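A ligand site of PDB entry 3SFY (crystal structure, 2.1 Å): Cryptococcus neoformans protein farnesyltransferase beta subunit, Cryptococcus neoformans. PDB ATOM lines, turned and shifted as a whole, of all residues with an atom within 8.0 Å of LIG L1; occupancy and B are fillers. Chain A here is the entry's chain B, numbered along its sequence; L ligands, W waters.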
ATOM      1  N   LEU A  50     -12.182   0.076 -36.662  1.00  0.00           N
ATOM      2  CA  LEU A  50     -13.203  -0.350 -35.692  1.00  0.00           C
ATOM      3  C   LEU A  50     -13.250  -1.878 -35.626  1.00  0.00           C
ATOM      4  O   LEU A  50     -13.170  -2.459 -34.530  1.00  0.00           O
ATOM      5  CB  LEU A  50     -14.593   0.176 -36.086  1.00  0.00           C
ATOM      6  CG  LEU A  50     -15.005   1.648 -35.947  1.00  0.00           C
ATOM      7  CD1 LEU A  50     -16.429   1.820 -36.457  1.00  0.00           C
ATOM      8  CD2 LEU A  50     -14.880   2.174 -34.523  1.00  0.00           C
ATOM      9  N   SER A  52     -11.565  -4.415 -35.298  1.00  0.00           N
ATOM     10  CA  SER A  52     -10.254  -4.827 -34.787  1.00  0.00           C
ATOM     11  C   SER A  52     -10.015  -6.293 -35.153  1.00  0.00           C
ATOM     12  O   SER A  52     -10.607  -7.200 -34.558  1.00  0.00           O
ATOM     13  CB  SER A  52     -10.160  -4.599 -33.276  1.00  0.00           C
ATOM     14  OG  SER A  52      -8.804  -4.666 -32.862  1.00  0.00           O
ATOM     15  N   TYR A  58      -3.075  -6.842 -31.549  1.00  0.00           N
ATOM     16  CA  TYR A  58      -3.646  -5.558 -31.146  1.00  0.00           C
ATOM     17  C   TYR A  58      -2.540  -4.557 -30.788  1.00  0.00           C
ATOM     18  O   TYR A  58      -1.675  -4.833 -29.956  1.00  0.00           O
ATOM     19  CB  TYR A  58      -4.680  -5.726 -30.003  1.00  0.00           C
ATOM     20  CG  TYR A  58      -5.291  -4.399 -29.583  1.00  0.00           C
ATOM     21  CD1 TYR A  58      -5.101  -3.905 -28.279  1.00  0.00           C
ATOM     22  CD2 TYR A  58      -6.035  -3.627 -30.484  1.00  0.00           C
ATOM     23  CE1 TYR A  58      -5.633  -2.662 -27.892  1.00  0.00           C
ATOM     24  CE2 TYR A  58      -6.574  -2.372 -30.103  1.00  0.00           C
ATOM     25  CZ  TYR A  58      -6.375  -1.908 -28.797  1.00  0.00           C
ATOM     26  OH  TYR A  58      -6.888  -0.670 -28.421  1.00  0.00           O
ATOM     27  N   GLY A  60      -2.679  -1.618 -29.252  1.00  0.00           N
ATOM     28  CA  GLY A  60      -2.881  -0.711 -28.120  1.00  0.00           C
ATOM     29  C   GLY A  60      -1.637  -0.500 -27.258  1.00  0.00           C
ATOM     30  O   GLY A  60      -0.869  -1.441 -27.015  1.00  0.00           O
ATOM     31  N   LEU A  61      -1.441   0.723 -26.786  1.00  0.00           N
ATOM     32  CA  LEU A  61      -0.277   1.032 -25.957  1.00  0.00           C
ATOM     33  C   LEU A  61      -0.352   0.210 -24.666  1.00  0.00           C
ATOM     34  O   LEU A  61      -1.334   0.304 -23.913  1.00  0.00           O
ATOM     35  CB  LEU A  61      -0.209   2.534 -25.649  1.00  0.00           C
ATOM     36  CG  LEU A  61       1.023   2.998 -24.846  1.00  0.00           C
ATOM     37  CD1 LEU A  61       2.305   2.850 -25.678  1.00  0.00           C
ATOM     38  CD2 LEU A  61       0.820   4.434 -24.377  1.00  0.00           C
ATOM     39  N   ILE A 486      -5.393  11.138 -31.207  1.00  0.00           N
ATOM     40  CA  ILE A 486      -5.002   9.922 -30.492  1.00  0.00           C
ATOM     41  C   ILE A 486      -5.336   8.694 -31.337  1.00  0.00           C
ATOM     42  O   ILE A 486      -6.472   8.171 -31.283  1.00  0.00           O
ATOM     43  CB  ILE A 486      -5.620   9.779 -29.077  1.00  0.00           C
ATOM     44  CG1 ILE A 486      -5.606  11.129 -28.316  1.00  0.00           C
ATOM     45  CG2 ILE A 486      -4.905   8.652 -28.283  1.00  0.00           C
ATOM     46  CD1 ILE A 486      -4.204  11.623 -27.943  1.00  0.00           C
ATOM     47  N   VAL A 487      -4.340   8.251 -32.105  1.00  0.00           N
ATOM     48  CA  VAL A 487      -4.462   7.082 -32.953  1.00  0.00           C
ATOM     49  C   VAL A 487      -4.774   5.857 -32.100  1.00  0.00           C
ATOM     50  O   VAL A 487      -4.108   5.617 -31.086  1.00  0.00           O
ATOM     51  CB  VAL A 487      -3.169   6.867 -33.802  1.00  0.00           C
ATOM     52  CG1 VAL A 487      -3.216   5.497 -34.548  1.00  0.00           C
ATOM     53  CG2 VAL A 487      -3.018   7.979 -34.814  1.00  0.00           C
ATOM     54  N   GLY A 488      -5.823   5.132 -32.480  1.00  0.00           N
ATOM     55  CA  GLY A 488      -6.213   3.889 -31.817  1.00  0.00           C
ATOM     56  C   GLY A 488      -7.153   4.069 -30.626  1.00  0.00           C
ATOM     57  O   GLY A 488      -7.518   3.082 -29.971  1.00  0.00           O
ATOM     58  N   GLY A 489      -7.544   5.312 -30.350  1.00  0.00           N
ATOM     59  CA  GLY A 489      -8.551   5.573 -29.316  1.00  0.00           C
ATOM     60  C   GLY A 489      -7.912   6.123 -28.052  1.00  0.00           C
ATOM     61  O   GLY A 489      -6.692   6.090 -27.869  1.00  0.00           O
ATOM     62  N   LYS A 490      -8.756   6.622 -27.151  1.00  0.00           N
ATOM     63  CA  LYS A 490      -8.268   7.480 -26.055  1.00  0.00           C
ATOM     64  C   LYS A 490      -7.458   6.743 -25.001  1.00  0.00           C
ATOM     65  O   LYS A 490      -6.684   7.367 -24.280  1.00  0.00           O
ATOM     66  CB  LYS A 490      -9.429   8.251 -25.423  1.00  0.00           C
ATOM     67  CG  LYS A 490      -9.933   9.338 -26.372  1.00  0.00           C
ATOM     68  CD  LYS A 490     -11.229   9.953 -25.874  1.00  0.00           C
ATOM     69  CE  LYS A 490     -11.485  11.309 -26.514  1.00  0.00           C
ATOM     70  NZ  LYS A 490     -12.869  11.750 -26.178  1.00  0.00           N
ATOM     71  N   ASP A 491      -7.604   5.423 -24.917  1.00  0.00           N
ATOM     72  CA  ASP A 491      -6.767   4.641 -23.999  1.00  0.00           C
ATOM     73  C   ASP A 491      -5.285   4.688 -24.382  1.00  0.00           C
ATOM     74  O   ASP A 491      -4.430   4.359 -23.553  1.00  0.00           O
ATOM     75  CB  ASP A 491      -7.246   3.190 -23.871  1.00  0.00           C
ATOM     76  CG  ASP A 491      -8.533   3.054 -23.079  1.00  0.00           C
ATOM     77  OD1 ASP A 491      -8.680   3.719 -22.025  1.00  0.00           O
ATOM     78  OD2 ASP A 491      -9.394   2.261 -23.469  1.00  0.00           O
ATOM     79  N   ASN A 492      -4.978   5.079 -25.624  1.00  0.00           N
ATOM     80  CA  ASN A 492      -3.564   5.286 -26.026  1.00  0.00           C
ATOM     81  C   ASN A 492      -2.980   6.631 -25.608  1.00  0.00           C
ATOM     82  O   ASN A 492      -1.764   6.845 -25.752  1.00  0.00           O
ATOM     83  CB  ASN A 492      -3.387   5.116 -27.537  1.00  0.00           C
ATOM     84  CG  ASN A 492      -3.549   3.668 -28.004  1.00  0.00           C
ATOM     85  OD1 ASN A 492      -3.426   2.714 -27.230  1.00  0.00           O
ATOM     86  ND2 ASN A 492      -3.803   3.493 -29.293  1.00  0.00           N
ATOM     87  N   ARG A 493      -3.821   7.553 -25.149  1.00  0.00           N
ATOM     88  CA  ARG A 493      -3.397   8.906 -24.792  1.00  0.00           C
ATOM     89  C   ARG A 493      -2.366   8.869 -23.669  1.00  0.00           C
ATOM     90  O   ARG A 493      -2.593   8.227 -22.623  1.00  0.00           O
ATOM     91  CB  ARG A 493      -4.570   9.758 -24.324  1.00  0.00           C
ATOM     92  CG  ARG A 493      -4.221  11.239 -24.114  1.00  0.00           C
ATOM     93  CD  ARG A 493      -5.155  11.891 -23.095  1.00  0.00           C
ATOM     94  NE  ARG A 493      -4.743  13.292 -22.897  1.00  0.00           N
ATOM     95  CZ  ARG A 493      -3.933  13.727 -21.937  1.00  0.00           C
ATOM     96  NH1 ARG A 493      -3.433  12.900 -21.027  1.00  0.00           N
ATOM     97  NH2 ARG A 493      -3.628  15.019 -21.881  1.00  0.00           N
HETATM   98  O1  LIG L   1     -13.832   6.320 -27.786  1.00  0.00           O
HETATM   99  O2  LIG L   1     -12.498   6.578 -25.784  1.00  0.00           O
HETATM  100  O3  LIG L   1     -10.432   4.337 -25.583  1.00  0.00           O
HETATM  101  O4  LIG L   1     -11.435   6.369 -27.999  1.00  0.00           O
HETATM  102  C1  LIG L   1      -9.836  -2.594 -24.548  1.00  0.00           C
HETATM  103  C2  LIG L   1     -11.241  -2.016 -24.823  1.00  0.00           C
HETATM  104  C3  LIG L   1      -8.817  -2.051 -25.568  1.00  0.00           C
HETATM  105  C4  LIG L   1     -11.230  -0.482 -24.938  1.00  0.00           C
HETATM  106  C5  LIG L   1      -8.768  -0.513 -25.462  1.00  0.00           C
HETATM  107  C6  LIG L   1     -11.090   2.165 -26.593  1.00  0.00           C
HETATM  108  C7  LIG L   1     -12.481   4.129 -27.018  1.00  0.00           C
HETATM  109  N1  LIG L   1     -10.027   1.523 -25.787  1.00  0.00           N
HETATM  110  C8  LIG L   1     -11.526   3.500 -26.003  1.00  0.00           C
HETATM  111  C9  LIG L   1     -10.116   0.058 -25.883  1.00  0.00           C
HETATM  112  S1  LIG L   1     -12.560   5.943 -27.145  1.00  0.00           S
HETATM  113  O1  LG2 L   2      -0.053  -3.143 -20.522  1.00  0.00           O
HETATM  114  O2  LG2 L   2      -1.045  -4.752 -22.057  1.00  0.00           O
HETATM  115  O3  LG2 L   2      -1.944  -6.933 -20.791  1.00  0.00           O
HETATM  116  O4  LG2 L   2      -2.418  -2.992 -21.008  1.00  0.00           O
HETATM  117  C1  LG2 L   2      -6.252 -10.660 -17.123  1.00  0.00           C
HETATM  118  C2  LG2 L   2      -4.782 -11.110 -17.105  1.00  0.00           C
HETATM  119  C3  LG2 L   2      -6.365  -9.163 -16.832  1.00  0.00           C
HETATM  120  C4  LG2 L   2      -3.897 -10.264 -18.052  1.00  0.00           C
HETATM  121  C5  LG2 L   2      -5.547  -8.346 -17.839  1.00  0.00           C
HETATM  122  C6  LG2 L   2      -2.177  -7.236 -18.370  1.00  0.00           C
HETATM  123  C7  LG2 L   2      -1.692  -4.973 -19.375  1.00  0.00           C
HETATM  124  N1  LG2 L   2      -3.341  -7.998 -18.889  1.00  0.00           N
HETATM  125  C8  LG2 L   2      -1.466  -6.477 -19.511  1.00  0.00           C
HETATM  126  C9  LG2 L   2      -4.054  -8.742 -17.813  1.00  0.00           C
HETATM  127  S1  LG2 L   2      -1.280  -3.917 -20.825  1.00  0.00           S
HETATM  128  O   HOH W   1      -7.780   2.703 -27.305  1.00  0.00           O
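The backbone NH (N) of Asp 491 lies within hydrogen-bond range of an oxygen (O3) of LIG L1, at 3.1 Å. A nitrogen (N1) of LIG L1 is in salt-bridge range of the side-chain carboxylate of Asp 491, at 2.5 Å. An oxygen (O4) of LIG L1 sits at hydrogen-bond distance from the backbone NH (N) of Lys 490, 2.8 Å away.
Water W1 lies within hydrogen-bond range of O of Gly 488 and N1 of LIG L1.
Residues that only touch LIG L1: Tyr 58 (3.5 Å) and Gly 489 (3.3 Å). Hydrophobic or aromatic side chains within 4 Å of LIG L1: Tyr 58. Four residues have an atom within 4 Å of LIG L1: Tyr 58, Gly 489, Lys 490 and Asp 491.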
